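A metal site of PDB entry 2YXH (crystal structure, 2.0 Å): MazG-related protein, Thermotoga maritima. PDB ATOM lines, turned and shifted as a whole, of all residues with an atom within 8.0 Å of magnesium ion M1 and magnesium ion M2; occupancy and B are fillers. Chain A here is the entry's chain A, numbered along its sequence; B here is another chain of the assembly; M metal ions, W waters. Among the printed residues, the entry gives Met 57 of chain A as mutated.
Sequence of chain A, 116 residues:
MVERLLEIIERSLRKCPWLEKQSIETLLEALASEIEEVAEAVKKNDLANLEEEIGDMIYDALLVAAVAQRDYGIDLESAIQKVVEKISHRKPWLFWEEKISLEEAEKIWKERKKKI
OD1 of Asp 56 is in salt-bridge range of NZ of Lys 86 of chain B (2.6 Å).
OE2 of Glu 53 sits close to OD1 of Asn 49.
Four residues have an atom within 4 Å of magnesium ion M1: Glu 34, Glu 37, Glu 53 and Asp 56.
The nearest printed residue that does not touch magnesium ion M1 is Glu 52 (4.1 Å).
Within 4 Å of magnesium ion M2: Glu 34 and Asp 60.
Magnesium ion M1 is bound by OD2 of Asp 56 (1.9 Å), OE2 of Glu 37 (2.0 Å), OE1 of Glu 53 (2.1 Å), OE1 of Glu 34 (2.2 Å), water W1 (2.3 Å) and water W2 (2.3 Å).
Magnesium ion M2 is bound by water W6 (2.0 Å), the side-chain carboxylate (OE2) of Glu 34 (2.0 Å), water W4 (2.1 Å), water W3 (2.1 Å), water W5 (2.2 Å) and the side-chain carboxylate (OD2) of Asp 60 (2.2 Å).
Water W2 bridges OE2 of Glu 53 (2.5 Å) and OE2 of Glu 52 (2.5 Å).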
ATOM      1  N   TRP A  18      22.586  -6.925 -17.434  1.00  0.00           N
ATOM      2  CA  TRP A  18      21.463  -7.581 -16.836  1.00  0.00           C
ATOM      3  C   TRP A  18      20.856  -6.634 -15.779  1.00  0.00           C
ATOM      4  O   TRP A  18      19.599  -6.441 -15.736  1.00  0.00           O
ATOM      5  CB  TRP A  18      21.881  -8.963 -16.250  1.00  0.00           C
ATOM      6  CG  TRP A  18      20.829  -9.565 -15.479  1.00  0.00           C
ATOM      7  CD1 TRP A  18      19.754 -10.330 -15.976  1.00  0.00           C
ATOM      8  CD2 TRP A  18      20.610  -9.428 -14.080  1.00  0.00           C
ATOM      9  NE1 TRP A  18      18.945 -10.693 -14.927  1.00  0.00           N
ATOM     10  CE2 TRP A  18      19.430 -10.144 -13.756  1.00  0.00           C
ATOM     11  CE3 TRP A  18      21.320  -8.794 -13.034  1.00  0.00           C
ATOM     12  CZ2 TRP A  18      18.966 -10.263 -12.443  1.00  0.00           C
ATOM     13  CZ3 TRP A  18      20.849  -8.902 -11.762  1.00  0.00           C
ATOM     14  CH2 TRP A  18      19.651  -9.613 -11.471  1.00  0.00           C
ATOM     15  N   LEU A  27      13.619  -6.772  -8.469  1.00  0.00           N
ATOM     16  CA  LEU A  27      14.588  -7.066  -7.467  1.00  0.00           C
ATOM     17  C   LEU A  27      13.932  -7.413  -6.126  1.00  0.00           C
ATOM     18  O   LEU A  27      14.407  -8.313  -5.385  1.00  0.00           O
ATOM     19  CB  LEU A  27      15.551  -5.910  -7.377  1.00  0.00           C
ATOM     20  CG  LEU A  27      16.325  -5.831  -8.690  1.00  0.00           C
ATOM     21  CD1 LEU A  27      17.262  -4.483  -8.779  1.00  0.00           C
ATOM     22  CD2 LEU A  27      17.044  -7.181  -8.912  1.00  0.00           C
ATOM     23  N   GLU A  29      11.127  -8.927  -5.733  1.00  0.00           N
ATOM     24  CA  GLU A  29      10.740 -10.376  -5.934  1.00  0.00           C
ATOM     25  C   GLU A  29      11.938 -11.287  -5.842  1.00  0.00           C
ATOM     26  O   GLU A  29      11.873 -12.284  -5.198  1.00  0.00           O
ATOM     27  CB  GLU A  29      10.166 -10.615  -7.348  1.00  0.00           C
ATOM     28  CG  GLU A  29       8.677 -10.576  -7.456  1.00  0.00           C
ATOM     29  CD  GLU A  29       8.192  -9.955  -8.784  1.00  0.00           C
ATOM     30  OE1 GLU A  29       8.743 -10.302  -9.879  1.00  0.00           O
ATOM     31  OE2 GLU A  29       7.242  -9.114  -8.737  1.00  0.00           O
ATOM     32  N   ALA A  30      13.067 -10.928  -6.454  1.00  0.00           N
ATOM     33  CA  ALA A  30      14.285 -11.739  -6.251  1.00  0.00           C
ATOM     34  C   ALA A  30      14.569 -11.871  -4.734  1.00  0.00           C
ATOM     35  O   ALA A  30      14.833 -12.954  -4.227  1.00  0.00           O
ATOM     36  CB  ALA A  30      15.441 -11.222  -7.008  1.00  0.00           C
ATOM     37  N   LEU A  31      14.421 -10.776  -4.024  1.00  0.00           N
ATOM     38  CA  LEU A  31      14.663 -10.812  -2.571  1.00  0.00           C
ATOM     39  C   LEU A  31      13.669 -11.665  -1.790  1.00  0.00           C
ATOM     40  O   LEU A  31      14.095 -12.391  -0.886  1.00  0.00           O
ATOM     41  CB  LEU A  31      14.701  -9.386  -1.966  1.00  0.00           C
ATOM     42  CG  LEU A  31      14.925  -9.312  -0.457  1.00  0.00           C
ATOM     43  CD1 LEU A  31      16.125 -10.112   0.052  1.00  0.00           C
ATOM     44  CD2 LEU A  31      14.958  -7.893  -0.069  1.00  0.00           C
ATOM     45  N   ALA A  32      12.378 -11.632  -2.165  1.00  0.00           N
ATOM     46  CA  ALA A  32      11.360 -12.432  -1.492  1.00  0.00           C
ATOM     47  C   ALA A  32      11.686 -13.864  -1.797  1.00  0.00           C
ATOM     48  O   ALA A  32      11.494 -14.738  -0.938  1.00  0.00           O
ATOM     49  CB  ALA A  32       9.940 -12.067  -1.928  1.00  0.00           C
ATOM     50  N   SER A  33      12.260 -14.126  -2.968  1.00  0.00           N
ATOM     51  CA  SER A  33      12.663 -15.488  -3.261  1.00  0.00           C
ATOM     52  C   SER A  33      13.756 -16.035  -2.391  1.00  0.00           C
ATOM     53  O   SER A  33      13.655 -17.186  -1.971  1.00  0.00           O
ATOM     54  CB  SER A  33      13.006 -15.716  -4.727  1.00  0.00           C
ATOM     55  OG  SER A  33      13.565 -17.000  -4.923  1.00  0.00           O
ATOM     56  N   GLU A  34      14.839 -15.225  -2.122  1.00  0.00           N
ATOM     57  CA  GLU A  34      15.916 -15.752  -1.323  1.00  0.00           C
ATOM     58  C   GLU A  34      15.479 -15.977   0.090  1.00  0.00           C
ATOM     59  O   GLU A  34      16.051 -16.793   0.777  1.00  0.00           O
ATOM     60  CB  GLU A  34      17.114 -14.773  -1.215  1.00  0.00           C
ATOM     61  CG  GLU A  34      17.699 -14.433  -2.475  1.00  0.00           C
ATOM     62  CD  GLU A  34      18.457 -15.598  -3.103  1.00  0.00           C
ATOM     63  OE1 GLU A  34      18.732 -16.593  -2.376  1.00  0.00           O
ATOM     64  OE2 GLU A  34      18.822 -15.492  -4.300  1.00  0.00           O
ATOM     65  N   ILE A  35      14.600 -15.116   0.581  1.00  0.00           N
ATOM     66  CA  ILE A  35      13.950 -15.299   1.855  1.00  0.00           C
ATOM     67  C   ILE A  35      13.370 -16.729   1.925  1.00  0.00           C
ATOM     68  O   ILE A  35      13.465 -17.400   2.940  1.00  0.00           O
ATOM     69  CB  ILE A  35      12.718 -14.343   1.969  1.00  0.00           C
ATOM     70  CG1 ILE A  35      13.110 -12.979   2.424  1.00  0.00           C
ATOM     71  CG2 ILE A  35      11.642 -14.909   2.977  1.00  0.00           C
ATOM     72  CD1 ILE A  35      11.930 -12.082   2.476  1.00  0.00           C
ATOM     73  N   GLU A  36      12.770 -17.197   0.850  1.00  0.00           N
ATOM     74  CA  GLU A  36      12.265 -18.564   0.859  1.00  0.00           C
ATOM     75  C   GLU A  36      13.375 -19.589   0.879  1.00  0.00           C
ATOM     76  O   GLU A  36      13.270 -20.629   1.541  1.00  0.00           O
ATOM     77  CB  GLU A  36      11.344 -18.821  -0.324  1.00  0.00           C
ATOM     78  CG  GLU A  36      10.021 -17.933  -0.316  1.00  0.00           C
ATOM     79  CD  GLU A  36       9.052 -18.176   0.901  1.00  0.00           C
ATOM     80  OE1 GLU A  36       9.222 -19.098   1.746  1.00  0.00           O
ATOM     81  OE2 GLU A  36       8.062 -17.425   1.010  1.00  0.00           O
ATOM     82  N   GLU A  37      14.509 -19.313   0.214  1.00  0.00           N
ATOM     83  CA  GLU A  37      15.596 -20.243   0.297  1.00  0.00           C
ATOM     84  C   GLU A  37      16.112 -20.310   1.695  1.00  0.00           C
ATOM     85  O   GLU A  37      16.534 -21.346   2.152  1.00  0.00           O
ATOM     86  CB  GLU A  37      16.657 -19.972  -0.738  1.00  0.00           C
ATOM     87  CG  GLU A  37      16.067 -19.928  -2.161  1.00  0.00           C
ATOM     88  CD  GLU A  37      17.150 -19.743  -3.216  1.00  0.00           C
ATOM     89  OE1 GLU A  37      16.956 -20.282  -4.301  1.00  0.00           O
ATOM     90  OE2 GLU A  37      18.219 -19.104  -2.986  1.00  0.00           O
ATOM     91  N   VAL A  38      15.999 -19.212   2.442  1.00  0.00           N
ATOM     92  CA  VAL A  38      16.595 -19.180   3.785  1.00  0.00           C
ATOM     93  C   VAL A  38      15.657 -20.029   4.709  1.00  0.00           C
ATOM     94  O   VAL A  38      16.098 -20.936   5.464  1.00  0.00           O
ATOM     95  CB  VAL A  38      16.731 -17.711   4.310  1.00  0.00           C
ATOM     96  CG1 VAL A  38      16.912 -17.709   5.760  1.00  0.00           C
ATOM     97  CG2 VAL A  38      17.936 -17.021   3.628  1.00  0.00           C
ATOM     98  N   ASN A  49      23.966 -24.612   3.472  1.00  0.00           N
ATOM     99  CA  ASN A  49      23.047 -23.947   2.586  1.00  0.00           C
ATOM    100  C   ASN A  49      22.538 -22.703   3.295  1.00  0.00           C
ATOM    101  O   ASN A  49      22.344 -21.688   2.665  1.00  0.00           O
ATOM    102  CB  ASN A  49      21.876 -24.844   2.187  1.00  0.00           C
ATOM    103  CG  ASN A  49      20.916 -24.164   1.154  1.00  0.00           C
ATOM    104  OD1 ASN A  49      21.336 -23.717   0.059  1.00  0.00           O
ATOM    105  ND2 ASN A  49      19.633 -24.129   1.486  1.00  0.00           N
ATOM    106  N   GLU A  52      25.116 -20.038   2.595  1.00  0.00           N
ATOM    107  CA  GLU A  52      24.833 -19.579   1.303  1.00  0.00           C
ATOM    108  C   GLU A  52      23.634 -18.633   1.185  1.00  0.00           C
ATOM    109  O   GLU A  52      23.771 -17.578   0.653  1.00  0.00           O
ATOM    110  CB  GLU A  52      24.723 -20.743   0.328  1.00  0.00           C
ATOM    111  CG  GLU A  52      24.659 -20.290  -1.228  1.00  0.00           C
ATOM    112  CD  GLU A  52      23.778 -21.238  -2.164  1.00  0.00           C
ATOM    113  OE1 GLU A  52      23.620 -22.443  -1.832  1.00  0.00           O
ATOM    114  OE2 GLU A  52      23.318 -20.771  -3.236  1.00  0.00           O
ATOM    115  N   GLU A  53      22.415 -19.058   1.537  1.00  0.00           N
ATOM    116  CA  GLU A  53      21.307 -18.209   1.367  1.00  0.00           C
ATOM    117  C   GLU A  53      21.395 -16.876   2.191  1.00  0.00           C
ATOM    118  O   GLU A  53      20.855 -15.844   1.767  1.00  0.00           O
ATOM    119  CB  GLU A  53      20.059 -19.016   1.728  1.00  0.00           C
ATOM    120  CG  GLU A  53      20.099 -20.407   1.007  1.00  0.00           C
ATOM    121  CD  GLU A  53      20.109 -20.243  -0.531  1.00  0.00           C
ATOM    122  OE1 GLU A  53      19.850 -19.125  -1.032  1.00  0.00           O
ATOM    123  OE2 GLU A  53      20.413 -21.205  -1.258  1.00  0.00           O
ATOM    124  N   ILE A  54      21.920 -16.946   3.406  1.00  0.00           N
ATOM    125  CA  ILE A  54      22.126 -15.661   4.148  1.00  0.00           C
ATOM    126  C   ILE A  54      22.904 -14.668   3.243  1.00  0.00           C
ATOM    127  O   ILE A  54      22.526 -13.509   3.037  1.00  0.00           O
ATOM    128  CB  ILE A  54      22.800 -15.883   5.515  1.00  0.00           C
ATOM    129  CG1 ILE A  54      21.783 -16.636   6.441  1.00  0.00           C
ATOM    130  CG2 ILE A  54      23.120 -14.502   6.156  1.00  0.00           C
ATOM    131  CD1 ILE A  54      20.462 -15.859   6.719  1.00  0.00           C
ATOM    132  N   GLY A  55      24.001 -15.172   2.646  1.00  0.00           N
ATOM    133  CA  GLY A  55      24.727 -14.294   1.756  1.00  0.00           C
ATOM    134  C   GLY A  55      23.892 -13.829   0.555  1.00  0.00           C
ATOM    135  O   GLY A  55      23.829 -12.622   0.252  1.00  0.00           O
ATOM    136  N   ASP A  56      23.247 -14.772  -0.139  1.00  0.00           N
ATOM    137  CA  ASP A  56      22.348 -14.414  -1.233  1.00  0.00           C
ATOM    138  C   ASP A  56      21.377 -13.334  -0.835  1.00  0.00           C
ATOM    139  O   ASP A  56      21.057 -12.447  -1.586  1.00  0.00           O
ATOM    140  CB  ASP A  56      21.557 -15.631  -1.613  1.00  0.00           C
ATOM    141  CG  ASP A  56      22.330 -16.582  -2.451  1.00  0.00           C
ATOM    142  OD1 ASP A  56      23.512 -16.376  -2.782  1.00  0.00           O
ATOM    143  OD2 ASP A  56      21.751 -17.512  -2.919  1.00  0.00           O
ATOM    144  N   MET A  57      20.835 -13.469   0.361  1.00  0.00           N
ATOM    145  CA  MET A  57      19.770 -12.642   0.849  1.00  0.00           C
ATOM    146  C   MET A  57      20.255 -11.212   1.052  1.00  0.00           C
ATOM    147  O   MET A  57      19.580 -10.262   0.697  1.00  0.00           O
ATOM    148  CB  MET A  57      19.289 -13.228   2.200  1.00  0.00           C
ATOM    149  CG  MET A  57      18.178 -12.323   2.836  1.00  0.00           C
ATOM    150  SD  MET A  57      17.801 -12.671   4.740  1.00  0.00           S
ATOM    151  CE  MET A  57      19.670 -12.256   5.478  1.00  0.00           C
ATOM    152  N   TYR A  59      23.054  -9.757  -0.293  1.00  0.00           N
ATOM    153  CA  TYR A  59      23.294  -9.265  -1.633  1.00  0.00           C
ATOM    154  C   TYR A  59      22.007  -8.749  -2.322  1.00  0.00           C
ATOM    155  O   TYR A  59      21.972  -7.639  -2.903  1.00  0.00           O
ATOM    156  CB  TYR A  59      23.927 -10.377  -2.415  1.00  0.00           C
ATOM    157  CG  TYR A  59      24.066 -10.148  -3.863  1.00  0.00           C
ATOM    158  CD1 TYR A  59      24.883  -9.104  -4.344  1.00  0.00           C
ATOM    159  CD2 TYR A  59      23.426 -10.992  -4.786  1.00  0.00           C
ATOM    160  CE1 TYR A  59      25.055  -8.895  -5.749  1.00  0.00           C
ATOM    161  CE2 TYR A  59      23.572 -10.768  -6.254  1.00  0.00           C
ATOM    162  CZ  TYR A  59      24.415  -9.739  -6.673  1.00  0.00           C
ATOM    163  OH  TYR A  59      24.625  -9.473  -8.012  1.00  0.00           O
ATOM    164  N   ASP A  60      20.977  -9.568  -2.309  1.00  0.00           N
ATOM    165  CA  ASP A  60      19.777  -9.156  -2.970  1.00  0.00           C
ATOM    166  C   ASP A  60      19.101  -7.962  -2.366  1.00  0.00           C
ATOM    167  O   ASP A  60      18.592  -7.124  -3.081  1.00  0.00           O
ATOM    168  CB  ASP A  60      18.825 -10.319  -3.049  1.00  0.00           C
ATOM    169  CG  ASP A  60      19.192 -11.305  -4.210  1.00  0.00           C
ATOM    170  OD1 ASP A  60      20.216 -11.142  -4.950  1.00  0.00           O
ATOM    171  OD2 ASP A  60      18.454 -12.281  -4.370  1.00  0.00           O
ATOM    172  N   ALA A  61      19.082  -7.856  -1.043  1.00  0.00           N
ATOM    173  CA  ALA A  61      18.567  -6.666  -0.394  1.00  0.00           C
ATOM    174  C   ALA A  61      19.423  -5.462  -0.835  1.00  0.00           C
ATOM    175  O   ALA A  61      18.951  -4.345  -1.082  1.00  0.00           O
ATOM    176  CB  ALA A  61      18.697  -6.800   1.058  1.00  0.00           C
ATOM    177  N   LEU A  63      21.071  -5.169  -3.578  1.00  0.00           N
ATOM    178  CA  LEU A  63      20.699  -4.802  -4.939  1.00  0.00           C
ATOM    179  C   LEU A  63      19.362  -4.029  -4.982  1.00  0.00           C
ATOM    180  O   LEU A  63      19.151  -3.203  -5.848  1.00  0.00           O
ATOM    181  CB  LEU A  63      20.560  -5.951  -5.864  1.00  0.00           C
ATOM    182  CG  LEU A  63      21.790  -6.567  -6.469  1.00  0.00           C
ATOM    183  CD1 LEU A  63      21.333  -7.819  -7.315  1.00  0.00           C
ATOM    184  CD2 LEU A  63      22.801  -5.519  -7.227  1.00  0.00           C
ATOM    185  N   VAL B  83      29.145 -15.231  -1.083  1.00  0.00           N
ATOM    186  CA  VAL B  83      28.308 -14.626  -2.110  1.00  0.00           C
ATOM    187  C   VAL B  83      29.226 -13.780  -2.985  1.00  0.00           C
ATOM    188  O   VAL B  83      29.079 -13.734  -4.136  1.00  0.00           O
ATOM    189  CB  VAL B  83      27.001 -13.921  -1.544  1.00  0.00           C
ATOM    190  CG1 VAL B  83      27.343 -12.645  -0.988  1.00  0.00           C
ATOM    191  CG2 VAL B  83      25.860 -13.742  -2.693  1.00  0.00           C
ATOM    192  N   LYS B  86      30.598 -16.266  -5.341  1.00  0.00           N
ATOM    193  CA  LYS B  86      29.610 -16.743  -6.271  1.00  0.00           C
ATOM    194  C   LYS B  86      29.391 -15.729  -7.437  1.00  0.00           C
ATOM    195  O   LYS B  86      29.460 -16.068  -8.604  1.00  0.00           O
ATOM    196  CB  LYS B  86      28.311 -17.051  -5.503  1.00  0.00           C
ATOM    197  CG  LYS B  86      27.168 -17.642  -6.362  1.00  0.00           C
ATOM    198  CD  LYS B  86      25.800 -17.372  -5.730  1.00  0.00           C
ATOM    199  CE  LYS B  86      25.233 -18.577  -5.071  1.00  0.00           C
ATOM    200  NZ  LYS B  86      23.923 -18.365  -4.480  1.00  0.00           N
ATOM    201  N   ARG B  90      30.045 -16.095 -11.364  1.00  0.00           N
ATOM    202  CA  ARG B  90      28.981 -15.992 -12.349  1.00  0.00           C
ATOM    203  C   ARG B  90      28.984 -14.782 -13.256  1.00  0.00           C
ATOM    204  O   ARG B  90      28.510 -14.897 -14.369  1.00  0.00           O
ATOM    205  CB  ARG B  90      27.613 -16.148 -11.691  1.00  0.00           C
ATOM    206  CG  ARG B  90      27.525 -17.432 -11.054  1.00  0.00           C
ATOM    207  CD  ARG B  90      26.130 -17.694 -10.610  1.00  0.00           C
ATOM    208  NE  ARG B  90      25.953 -18.998  -9.990  1.00  0.00           N
ATOM    209  CZ  ARG B  90      24.813 -19.406  -9.377  1.00  0.00           C
ATOM    210  NH1 ARG B  90      23.770 -18.585  -9.224  1.00  0.00           N
ATOM    211  NH2 ARG B  90      24.757 -20.642  -8.881  1.00  0.00           N
HETATM  212 MG    MG M   1      20.050 -18.308  -2.912  1.00  0.00          MG
HETATM  213 MG    MG M   2      18.947 -14.016  -5.700  1.00  0.00          MG
HETATM  214  O   HOH W   1      19.958 -17.684  -5.101  1.00  0.00           O
HETATM  215  O   HOH W   2      20.833 -20.392  -3.565  1.00  0.00           O
HETATM  216  O   HOH W   3      21.056 -13.836  -5.699  1.00  0.00           O
HETATM  217  O   HOH W   4      18.484 -12.772  -7.307  1.00  0.00           O
HETATM  218  O   HOH W   5      18.794 -15.606  -7.156  1.00  0.00           O
HETATM  219  O   HOH W   6      16.966 -14.291  -5.675  1.00  0.00           O
